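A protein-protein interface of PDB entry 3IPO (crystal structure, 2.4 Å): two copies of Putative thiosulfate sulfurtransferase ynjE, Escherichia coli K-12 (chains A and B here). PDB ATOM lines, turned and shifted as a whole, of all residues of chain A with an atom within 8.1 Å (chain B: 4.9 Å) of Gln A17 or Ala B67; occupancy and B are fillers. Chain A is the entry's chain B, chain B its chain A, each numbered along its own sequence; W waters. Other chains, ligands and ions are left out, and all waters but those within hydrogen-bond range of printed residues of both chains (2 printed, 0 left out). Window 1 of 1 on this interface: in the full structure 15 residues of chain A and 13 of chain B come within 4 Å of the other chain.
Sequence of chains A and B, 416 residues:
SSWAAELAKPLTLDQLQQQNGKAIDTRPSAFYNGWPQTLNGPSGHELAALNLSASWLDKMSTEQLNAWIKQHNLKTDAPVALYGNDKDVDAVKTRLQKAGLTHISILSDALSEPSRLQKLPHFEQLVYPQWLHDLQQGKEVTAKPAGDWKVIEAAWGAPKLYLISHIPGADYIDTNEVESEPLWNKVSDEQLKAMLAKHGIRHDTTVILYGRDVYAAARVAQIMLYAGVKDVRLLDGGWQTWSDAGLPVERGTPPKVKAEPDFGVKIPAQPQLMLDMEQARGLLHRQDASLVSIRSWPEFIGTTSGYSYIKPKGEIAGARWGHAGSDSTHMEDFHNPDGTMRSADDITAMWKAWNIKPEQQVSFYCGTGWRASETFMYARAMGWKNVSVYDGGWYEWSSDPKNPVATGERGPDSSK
OE2 of Glu B63 lies close to O of Gly A21, 2.7 Å away.
OD1 of Asn A20 lies within hydrogen-bond range of N of Glu B63 (3.1 Å).
OG of Ser B61 is in hydrogen-bond range of O of Gln A17 (2.7 Å).
The side-chain hydroxyl (OG) of Ser B61 is in hydrogen-bond range of the side-chain amide oxygen (OD1) of Asn A20 (3.4 Å).
N of Ser B61 lies within hydrogen-bond range of OE1 of Gln B64 (2.9 Å).
O of Leu A16 is in hydrogen-bond range of N of Gly A21.
The side-chain hydroxyl of Ser B61 lies close to the backbone NH of Glu B63, 3.4 Å away.
OE1 of Glu B63 touches O of Leu A16, 3.9 Å away.
CB of Glu B63 touches O of Gln A17 (3.4 Å).
Gln A17 touches Gln B64 (C to CG, 3.9 Å).
Gln A17 touches Ala B67 (OE1 to CB, 3.5 Å).
O of Gln A18 touches CB of Ser B61, at 3.5 Å.
CD of Gln B64 touches CA of Gln A18, 3.6 Å away.
ND2 of Asn B66 touches CD2 of Leu A47 (3.7 Å).
Leu A47 touches Ala B67.
Lys B70 touches Leu A47 (CG to CD2, 3.9 Å).
Gln A118 touches Lys B70 (NE2 to NZ, 3.9 Å).
Of chain B, only Ser B61, Glu B63, Gln B64 and Ala B67 come within 4 Å of Gln A17.
Printed residues of chain A within 4 Å of Ala B67: Gln A17 (3.5 Å) and Leu A47 (3.7 Å).
Of the printed residues of chain B, Leu A47 touches Asn B66 (3.7 Å), Ala B67 (3.7 Å) and Lys B70 (3.9 Å).
Of the printed residues of chain A, Asn B66 touches Leu A47 (3.7 Å).
Of the printed residues of chain A, Ser B61 touches Gln A17 (2.7 Å), Gln A18 (3.5 Å) and Asn A20 (3.4 Å).
Of the printed residues of chain B, Gln A118 touches Lys B70 (3.9 Å).
Printed residues of chain A within 4 Å of Lys B70: Leu A47 (3.9 Å) and Gln A118 (3.9 Å).
The nearest printed residue of chain A that does not touch Lys B70 is Arg A116 (6.5 Å).
Printed residues of chain B that touch a printed residue of chain A: Ser B61, Glu B63, Gln B64, Asn B66, Ala B67 and Lys B70.
Hydrophobic or aromatic side chains of chain B within 4 Å of the printed part of chain A: Ala B67.
Of the 22 printed residues of chain A, 7 touch a printed residue of chain B.
Among the printed residues, 14 pairs touch across the chains.
No position is printed for both chains.
Of the 14 pairs that touch across the chains among the printed residues, none has its exchanged pair printed and touching as well.
Water W1 bridges OE1 of Gln B64 and NE2 of Gln A18.
Water W2 bridges O of Asp A14 (2.9 Å) and NE2 of Gln B64 (3.1 Å).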
ATOM      1  N   LEU A  11       4.075  21.562  26.255  1.00  0.00           N
ATOM      2  CA  LEU A  11       5.217  20.870  25.652  1.00  0.00           C
ATOM      3  C   LEU A  11       5.733  21.690  24.470  1.00  0.00           C
ATOM      4  O   LEU A  11       4.924  22.220  23.653  1.00  0.00           O
ATOM      5  CB  LEU A  11       4.812  19.465  25.125  1.00  0.00           C
ATOM      6  CG  LEU A  11       4.475  18.283  26.061  1.00  0.00           C
ATOM      7  CD1 LEU A  11       4.152  16.975  25.323  1.00  0.00           C
ATOM      8  CD2 LEU A  11       5.552  17.973  27.029  1.00  0.00           C
ATOM      9  N   THR A  12       7.051  21.769  24.323  1.00  0.00           N
ATOM     10  CA  THR A  12       7.585  22.313  23.065  1.00  0.00           C
ATOM     11  C   THR A  12       7.421  21.277  21.940  1.00  0.00           C
ATOM     12  O   THR A  12       7.271  20.067  22.199  1.00  0.00           O
ATOM     13  CB  THR A  12       9.067  22.664  23.164  1.00  0.00           C
ATOM     14  OG1 THR A  12       9.786  21.440  23.233  1.00  0.00           O
ATOM     15  CG2 THR A  12       9.358  23.535  24.390  1.00  0.00           C
ATOM     16  N   LEU A  13       7.407  21.739  20.696  1.00  0.00           N
ATOM     17  CA  LEU A  13       7.416  20.782  19.593  1.00  0.00           C
ATOM     18  C   LEU A  13       8.572  19.746  19.705  1.00  0.00           C
ATOM     19  O   LEU A  13       8.346  18.563  19.471  1.00  0.00           O
ATOM     20  CB  LEU A  13       7.438  21.480  18.241  1.00  0.00           C
ATOM     21  CG  LEU A  13       7.287  20.551  17.001  1.00  0.00           C
ATOM     22  CD1 LEU A  13       5.891  19.943  16.871  1.00  0.00           C
ATOM     23  CD2 LEU A  13       7.617  21.354  15.761  1.00  0.00           C
ATOM     24  N   ASP A  14       9.780  20.203  20.074  1.00  0.00           N
ATOM     25  CA  ASP A  14      10.927  19.320  20.274  1.00  0.00           C
ATOM     26  C   ASP A  14      10.545  18.186  21.247  1.00  0.00           C
ATOM     27  O   ASP A  14      10.876  17.015  21.026  1.00  0.00           O
ATOM     28  CB  ASP A  14      12.180  20.047  20.834  1.00  0.00           C
ATOM     29  CG  ASP A  14      12.884  20.999  19.809  1.00  0.00           C
ATOM     30  OD1 ASP A  14      12.445  21.158  18.600  1.00  0.00           O
ATOM     31  OD2 ASP A  14      13.927  21.621  20.260  1.00  0.00           O
ATOM     32  N   GLN A  15       9.876  18.562  22.325  1.00  0.00           N
ATOM     33  CA  GLN A  15       9.407  17.601  23.337  1.00  0.00           C
ATOM     34  C   GLN A  15       8.317  16.670  22.798  1.00  0.00           C
ATOM     35  O   GLN A  15       8.401  15.470  22.956  1.00  0.00           O
ATOM     36  CB  GLN A  15       8.962  18.311  24.628  1.00  0.00           C
ATOM     37  CG  GLN A  15      10.141  18.736  25.512  1.00  0.00           C
ATOM     38  CD  GLN A  15       9.752  19.784  26.564  1.00  0.00           C
ATOM     39  OE1 GLN A  15       8.709  20.445  26.466  1.00  0.00           O
ATOM     40  NE2 GLN A  15      10.601  19.942  27.572  1.00  0.00           N
ATOM     41  N   LEU A  16       7.336  17.219  22.116  1.00  0.00           N
ATOM     42  CA  LEU A  16       6.265  16.418  21.537  1.00  0.00           C
ATOM     43  C   LEU A  16       6.874  15.347  20.608  1.00  0.00           C
ATOM     44  O   LEU A  16       6.505  14.176  20.672  1.00  0.00           O
ATOM     45  CB  LEU A  16       5.280  17.293  20.768  1.00  0.00           C
ATOM     46  CG  LEU A  16       3.993  16.624  20.316  1.00  0.00           C
ATOM     47  CD1 LEU A  16       3.122  16.266  21.537  1.00  0.00           C
ATOM     48  CD2 LEU A  16       3.253  17.592  19.382  1.00  0.00           C
ATOM     49  N   GLN A  17       7.821  15.784  19.779  1.00  0.00           N
ATOM     50  CA  GLN A  17       8.509  14.926  18.819  1.00  0.00           C
ATOM     51  C   GLN A  17       9.387  13.856  19.491  1.00  0.00           C
ATOM     52  O   GLN A  17       9.335  12.703  19.105  1.00  0.00           O
ATOM     53  CB  GLN A  17       9.286  15.774  17.781  1.00  0.00           C
ATOM     54  CG  GLN A  17       8.360  16.564  16.877  1.00  0.00           C
ATOM     55  CD  GLN A  17       9.087  17.578  15.984  1.00  0.00           C
ATOM     56  OE1 GLN A  17      10.193  18.033  16.307  1.00  0.00           O
ATOM     57  NE2 GLN A  17       8.463  17.924  14.848  1.00  0.00           N
ATOM     58  N   GLN A  18      10.158  14.232  20.504  1.00  0.00           N
ATOM     59  CA  GLN A  18      10.883  13.263  21.343  1.00  0.00           C
ATOM     60  C   GLN A  18       9.936  12.129  21.778  1.00  0.00           C
ATOM     61  O   GLN A  18      10.316  10.947  21.796  1.00  0.00           O
ATOM     62  CB  GLN A  18      11.474  13.965  22.588  1.00  0.00           C
ATOM     63  CG  GLN A  18      12.647  13.250  23.325  1.00  0.00           C
ATOM     64  CD  GLN A  18      12.200  11.980  24.111  1.00  0.00           C
ATOM     65  OE1 GLN A  18      11.178  12.001  24.809  1.00  0.00           O
ATOM     66  NE2 GLN A  18      12.968  10.872  23.988  1.00  0.00           N
ATOM     67  N   GLN A  19       8.712  12.485  22.135  1.00  0.00           N
ATOM     68  CA  GLN A  19       7.753  11.507  22.672  1.00  0.00           C
ATOM     69  C   GLN A  19       6.811  10.960  21.608  1.00  0.00           C
ATOM     70  O   GLN A  19       5.834  10.301  21.936  1.00  0.00           O
ATOM     71  CB  GLN A  19       6.947  12.145  23.812  1.00  0.00           C
ATOM     72  CG  GLN A  19       7.798  12.399  25.064  1.00  0.00           C
ATOM     73  CD  GLN A  19       7.202  13.462  26.015  1.00  0.00           C
ATOM     74  OE1 GLN A  19       7.884  14.439  26.414  1.00  0.00           O
ATOM     75  NE2 GLN A  19       5.940  13.272  26.381  1.00  0.00           N
ATOM     76  N   ASN A  20       7.057  11.264  20.334  1.00  0.00           N
ATOM     77  CA  ASN A  20       6.211  10.733  19.282  1.00  0.00           C
ATOM     78  C   ASN A  20       4.749  11.065  19.512  1.00  0.00           C
ATOM     79  O   ASN A  20       3.891  10.239  19.205  1.00  0.00           O
ATOM     80  CB  ASN A  20       6.364   9.193  19.144  1.00  0.00           C
ATOM     81  CG  ASN A  20       7.627   8.801  18.434  1.00  0.00           C
ATOM     82  OD1 ASN A  20       8.185   9.613  17.662  1.00  0.00           O
ATOM     83  ND2 ASN A  20       8.097   7.549  18.653  1.00  0.00           N
ATOM     84  N   GLY A  21       4.470  12.268  20.022  1.00  0.00           N
ATOM     85  CA  GLY A  21       3.091  12.748  20.225  1.00  0.00           C
ATOM     86  C   GLY A  21       2.487  13.335  18.963  1.00  0.00           C
ATOM     87  O   GLY A  21       3.117  13.305  17.893  1.00  0.00           O
ATOM     88  N   LYS A  22       1.270  13.852  19.094  1.00  0.00           N
ATOM     89  CA  LYS A  22       0.557  14.497  18.022  1.00  0.00           C
ATOM     90  C   LYS A  22       0.188  15.974  18.291  1.00  0.00           C
ATOM     91  O   LYS A  22      -0.352  16.310  19.355  1.00  0.00           O
ATOM     92  CB  LYS A  22      -0.734  13.740  17.769  1.00  0.00           C
ATOM     93  CG  LYS A  22      -0.671  12.966  16.491  1.00  0.00           C
ATOM     94  CD  LYS A  22      -0.307  11.548  16.756  1.00  0.00           C
ATOM     95  CE  LYS A  22      -0.757  10.652  15.578  1.00  0.00           C
ATOM     96  NZ  LYS A  22      -0.755   9.220  16.030  1.00  0.00           N
ATOM     97  N   ALA A  23       0.422  16.835  17.321  1.00  0.00           N
ATOM     98  CA  ALA A  23      -0.008  18.210  17.457  1.00  0.00           C
ATOM     99  C   ALA A  23      -1.355  18.357  16.796  1.00  0.00           C
ATOM    100  O   ALA A  23      -1.620  17.713  15.772  1.00  0.00           O
ATOM    101  CB  ALA A  23       0.978  19.107  16.802  1.00  0.00           C
ATOM    102  N   GLU A  46       2.379  23.085  12.037  1.00  0.00           N
ATOM    103  CA  GLU A  46       3.541  22.385  12.502  1.00  0.00           C
ATOM    104  C   GLU A  46       3.594  20.997  11.835  1.00  0.00           C
ATOM    105  O   GLU A  46       2.541  20.411  11.459  1.00  0.00           O
ATOM    106  CB  GLU A  46       3.523  22.262  14.034  1.00  0.00           C
ATOM    107  CG  GLU A  46       3.589  23.593  14.764  1.00  0.00           C
ATOM    108  CD  GLU A  46       4.924  24.339  14.636  1.00  0.00           C
ATOM    109  OE1 GLU A  46       5.875  23.879  13.960  1.00  0.00           O
ATOM    110  OE2 GLU A  46       5.044  25.414  15.258  1.00  0.00           O
ATOM    111  N   LEU A  47       4.825  20.499  11.657  1.00  0.00           N
ATOM    112  CA  LEU A  47       5.051  19.262  10.916  1.00  0.00           C
ATOM    113  C   LEU A  47       4.135  18.146  11.420  1.00  0.00           C
ATOM    114  O   LEU A  47       4.223  17.787  12.605  1.00  0.00           O
ATOM    115  CB  LEU A  47       6.508  18.815  10.994  1.00  0.00           C
ATOM    116  CG  LEU A  47       6.880  17.454  10.359  1.00  0.00           C
ATOM    117  CD1 LEU A  47       6.544  17.448   8.872  1.00  0.00           C
ATOM    118  CD2 LEU A  47       8.381  17.239  10.535  1.00  0.00           C
ATOM    119  N   ALA A  48       3.318  17.569  10.512  1.00  0.00           N
ATOM    120  CA  ALA A  48       2.472  16.388  10.860  1.00  0.00           C
ATOM    121  C   ALA A  48       1.328  16.718  11.843  1.00  0.00           C
ATOM    122  O   ALA A  48       0.708  15.822  12.365  1.00  0.00           O
ATOM    123  CB  ALA A  48       3.366  15.110  11.429  1.00  0.00           C
ATOM    124  N   ALA A  49       1.076  17.998  12.118  1.00  0.00           N
ATOM    125  CA  ALA A  49      -0.048  18.375  12.948  1.00  0.00           C
ATOM    126  C   ALA A  49      -1.283  17.883  12.251  1.00  0.00           C
ATOM    127  O   ALA A  49      -1.362  17.900  11.011  1.00  0.00           O
ATOM    128  CB  ALA A  49      -0.121  19.902  13.097  1.00  0.00           C
ATOM    129  N   PRO A  79       1.053  11.533  24.112  1.00  0.00           N
ATOM    130  CA  PRO A  79       0.825  12.984  24.284  1.00  0.00           C
ATOM    131  C   PRO A  79       0.205  13.665  23.036  1.00  0.00           C
ATOM    132  O   PRO A  79       0.578  13.373  21.895  1.00  0.00           O
ATOM    133  CB  PRO A  79       2.213  13.548  24.637  1.00  0.00           C
ATOM    134  CG  PRO A  79       3.189  12.513  24.051  1.00  0.00           C
ATOM    135  CD  PRO A  79       2.489  11.170  24.135  1.00  0.00           C
ATOM    136  N   LEU A 107       0.733  23.154  22.896  1.00  0.00           N
ATOM    137  CA  LEU A 107       2.023  23.228  22.219  1.00  0.00           C
ATOM    138  C   LEU A 107       2.568  24.637  22.431  1.00  0.00           C
ATOM    139  O   LEU A 107       2.136  25.589  21.765  1.00  0.00           O
ATOM    140  CB  LEU A 107       1.867  22.932  20.720  1.00  0.00           C
ATOM    141  CG  LEU A 107       3.166  22.802  19.896  1.00  0.00           C
ATOM    142  CD1 LEU A 107       4.009  21.662  20.407  1.00  0.00           C
ATOM    143  CD2 LEU A 107       2.859  22.576  18.410  1.00  0.00           C
ATOM    144  N   ASP A 109       5.273  26.344  21.913  1.00  0.00           N
ATOM    145  CA  ASP A 109       6.008  27.143  20.936  1.00  0.00           C
ATOM    146  C   ASP A 109       5.393  27.036  19.549  1.00  0.00           C
ATOM    147  O   ASP A 109       6.093  27.249  18.549  1.00  0.00           O
ATOM    148  CB  ASP A 109       7.510  26.776  20.903  1.00  0.00           C
ATOM    149  CG  ASP A 109       7.748  25.335  20.430  1.00  0.00           C
ATOM    150  OD1 ASP A 109       6.814  24.505  20.528  1.00  0.00           O
ATOM    151  OD2 ASP A 109       8.851  25.041  19.941  1.00  0.00           O
ATOM    152  N   ARG A 116       9.762  26.173   9.713  1.00  0.00           N
ATOM    153  CA  ARG A 116       9.484  24.739   9.878  1.00  0.00           C
ATOM    154  C   ARG A 116       8.001  24.445   9.617  1.00  0.00           C
ATOM    155  O   ARG A 116       7.568  23.329   9.856  1.00  0.00           O
ATOM    156  CB  ARG A 116       9.934  24.223  11.289  1.00  0.00           C
ATOM    157  CG  ARG A 116       9.039  24.688  12.440  1.00  0.00           C
ATOM    158  CD  ARG A 116       9.518  24.348  13.845  1.00  0.00           C
ATOM    159  NE  ARG A 116       8.419  24.587  14.794  1.00  0.00           N
ATOM    160  CZ  ARG A 116       8.578  24.836  16.090  1.00  0.00           C
ATOM    161  NH1 ARG A 116       9.778  24.886  16.594  1.00  0.00           N
ATOM    162  NH2 ARG A 116       7.542  25.041  16.887  1.00  0.00           N
ATOM    163  N   GLN A 118       4.388  23.743   7.545  1.00  0.00           N
ATOM    164  CA  GLN A 118       4.056  23.014   6.327  1.00  0.00           C
ATOM    165  C   GLN A 118       2.755  23.567   5.885  1.00  0.00           C
ATOM    166  O   GLN A 118       1.912  23.893   6.726  1.00  0.00           O
ATOM    167  CB  GLN A 118       3.851  21.513   6.600  1.00  0.00           C
ATOM    168  CG  GLN A 118       4.992  20.831   7.290  1.00  0.00           C
ATOM    169  CD  GLN A 118       6.235  20.754   6.425  1.00  0.00           C
ATOM    170  OE1 GLN A 118       7.275  21.306   6.775  1.00  0.00           O
ATOM    171  NE2 GLN A 118       6.136  20.060   5.301  1.00  0.00           N
ATOM    172  N   SER B  61      13.957   9.764  18.229  1.00  0.00           N
ATOM    173  CA  SER B  61      12.704   9.048  18.003  1.00  0.00           C
ATOM    174  C   SER B  61      12.347   9.175  16.511  1.00  0.00           C
ATOM    175  O   SER B  61      12.991   9.947  15.751  1.00  0.00           O
ATOM    176  CB  SER B  61      11.611   9.707  18.823  1.00  0.00           C
ATOM    177  OG  SER B  61      11.293  10.985  18.241  1.00  0.00           O
ATOM    178  N   GLU B  63       9.724  10.701  15.214  1.00  0.00           N
ATOM    179  CA  GLU B  63       9.352  12.081  14.957  1.00  0.00           C
ATOM    180  C   GLU B  63      10.550  13.037  14.997  1.00  0.00           C
ATOM    181  O   GLU B  63      10.604  14.010  14.206  1.00  0.00           O
ATOM    182  CB  GLU B  63       8.215  12.523  15.871  1.00  0.00           C
ATOM    183  CG  GLU B  63       6.912  11.778  15.575  1.00  0.00           C
ATOM    184  CD  GLU B  63       5.733  12.361  16.334  1.00  0.00           C
ATOM    185  OE1 GLU B  63       5.898  13.454  16.939  1.00  0.00           O
ATOM    186  OE2 GLU B  63       4.650  11.724  16.353  1.00  0.00           O
ATOM    187  N   GLN B  64      11.547  12.750  15.826  1.00  0.00           N
ATOM    188  CA  GLN B  64      12.740  13.613  15.788  1.00  0.00           C
ATOM    189  C   GLN B  64      13.481  13.542  14.464  1.00  0.00           C
ATOM    190  O   GLN B  64      13.868  14.591  13.905  1.00  0.00           O
ATOM    191  CB  GLN B  64      13.688  13.369  16.953  1.00  0.00           C
ATOM    192  CG  GLN B  64      13.087  13.804  18.237  1.00  0.00           C
ATOM    193  CD  GLN B  64      13.947  13.474  19.423  1.00  0.00           C
ATOM    194  OE1 GLN B  64      14.334  12.318  19.641  1.00  0.00           O
ATOM    195  NE2 GLN B  64      14.253  14.490  20.210  1.00  0.00           N
ATOM    196  N   LEU B  65      13.650  12.316  13.965  1.00  0.00           N
ATOM    197  CA  LEU B  65      14.303  12.060  12.681  1.00  0.00           C
ATOM    198  C   LEU B  65      13.521  12.687  11.516  1.00  0.00           C
ATOM    199  O   LEU B  65      14.121  13.330  10.632  1.00  0.00           O
ATOM    200  CB  LEU B  65      14.542  10.538  12.455  1.00  0.00           C
ATOM    201  CG  LEU B  65      15.280  10.210  11.142  1.00  0.00           C
ATOM    202  CD1 LEU B  65      16.570  11.029  11.004  1.00  0.00           C
ATOM    203  CD2 LEU B  65      15.575   8.731  11.055  1.00  0.00           C
ATOM    204  N   ASN B  66      12.199  12.506  11.525  1.00  0.00           N
ATOM    205  CA  ASN B  66      11.329  13.105  10.517  1.00  0.00           C
ATOM    206  C   ASN B  66      11.490  14.640  10.512  1.00  0.00           C
ATOM    207  O   ASN B  66      11.544  15.273   9.446  1.00  0.00           O
ATOM    208  CB  ASN B  66       9.867  12.688  10.776  1.00  0.00           C
ATOM    209  CG  ASN B  66       8.960  13.000   9.621  1.00  0.00           C
ATOM    210  OD1 ASN B  66       9.285  12.719   8.477  1.00  0.00           O
ATOM    211  ND2 ASN B  66       7.806  13.587   9.910  1.00  0.00           N
ATOM    212  N   ALA B  67      11.598  15.231  11.711  1.00  0.00           N
ATOM    213  CA  ALA B  67      11.755  16.672  11.824  1.00  0.00           C
ATOM    214  C   ALA B  67      13.119  17.101  11.290  1.00  0.00           C
ATOM    215  O   ALA B  67      13.252  18.164  10.663  1.00  0.00           O
ATOM    216  CB  ALA B  67      11.576  17.142  13.266  1.00  0.00           C
ATOM    217  N   TRP B  68      14.132  16.298  11.576  1.00  0.00           N
ATOM    218  CA  TRP B  68      15.493  16.606  11.128  1.00  0.00           C
ATOM    219  C   TRP B  68      15.544  16.484   9.576  1.00  0.00           C
ATOM    220  O   TRP B  68      16.133  17.315   8.899  1.00  0.00           O
ATOM    221  CB  TRP B  68      16.492  15.682  11.829  1.00  0.00           C
ATOM    222  CG  TRP B  68      17.942  15.943  11.482  1.00  0.00           C
ATOM    223  CD1 TRP B  68      18.856  16.639  12.236  1.00  0.00           C
ATOM    224  CD2 TRP B  68      18.645  15.477  10.308  1.00  0.00           C
ATOM    225  NE1 TRP B  68      20.076  16.669  11.577  1.00  0.00           N
ATOM    226  CE2 TRP B  68      19.965  15.980  10.388  1.00  0.00           C
ATOM    227  CE3 TRP B  68      18.279  14.688   9.198  1.00  0.00           C
ATOM    228  CZ2 TRP B  68      20.953  15.713   9.382  1.00  0.00           C
ATOM    229  CZ3 TRP B  68      19.250  14.422   8.186  1.00  0.00           C
ATOM    230  CH2 TRP B  68      20.574  14.940   8.296  1.00  0.00           C
ATOM    231  N   ILE B  69      14.876  15.472   9.025  1.00  0.00           N
ATOM    232  CA  ILE B  69      14.844  15.313   7.593  1.00  0.00           C
ATOM    233  C   ILE B  69      14.248  16.560   6.935  1.00  0.00           C
ATOM    234  O   ILE B  69      14.887  17.136   6.016  1.00  0.00           O
ATOM    235  CB  ILE B  69      14.092  14.037   7.183  1.00  0.00           C
ATOM    236  CG1 ILE B  69      14.991  12.796   7.387  1.00  0.00           C
ATOM    237  CG2 ILE B  69      13.612  14.121   5.721  1.00  0.00           C
ATOM    238  CD1 ILE B  69      14.185  11.512   7.443  1.00  0.00           C
ATOM    239  N   LYS B  70      13.048  16.968   7.405  1.00  0.00           N
ATOM    240  CA  LYS B  70      12.374  18.153   6.872  1.00  0.00           C
ATOM    241  C   LYS B  70      13.163  19.418   7.043  1.00  0.00           C
ATOM    242  O   LYS B  70      13.253  20.225   6.137  1.00  0.00           O
ATOM    243  CB  LYS B  70      11.031  18.379   7.560  1.00  0.00           C
ATOM    244  CG  LYS B  70       9.928  17.556   7.008  1.00  0.00           C
ATOM    245  CD  LYS B  70       9.582  17.948   5.542  1.00  0.00           C
ATOM    246  CE  LYS B  70       8.746  16.823   4.888  1.00  0.00           C
ATOM    247  NZ  LYS B  70       8.174  17.250   3.553  1.00  0.00           N
ATOM    248  N   GLN B  71      13.706  19.617   8.226  1.00  0.00           N
ATOM    249  CA  GLN B  71      14.441  20.804   8.494  1.00  0.00           C
ATOM    250  C   GLN B  71      15.696  20.970   7.631  1.00  0.00           C
ATOM    251  O   GLN B  71      16.214  22.085   7.516  1.00  0.00           O
ATOM    252  CB  GLN B  71      14.847  20.795   9.947  1.00  0.00           C
ATOM    253  CG  GLN B  71      15.950  21.749  10.295  1.00  0.00           C
ATOM    254  CD  GLN B  71      16.318  21.621  11.757  1.00  0.00           C
ATOM    255  OE1 GLN B  71      16.878  20.587  12.205  1.00  0.00           O
ATOM    256  NE2 GLN B  71      15.951  22.642  12.539  1.00  0.00           N
HETATM  257  O   HOH W   1      14.697  10.453  21.730  1.00  0.00           O
HETATM  258  O   HOH W   2      13.424  17.418  19.744  1.00  0.00           O
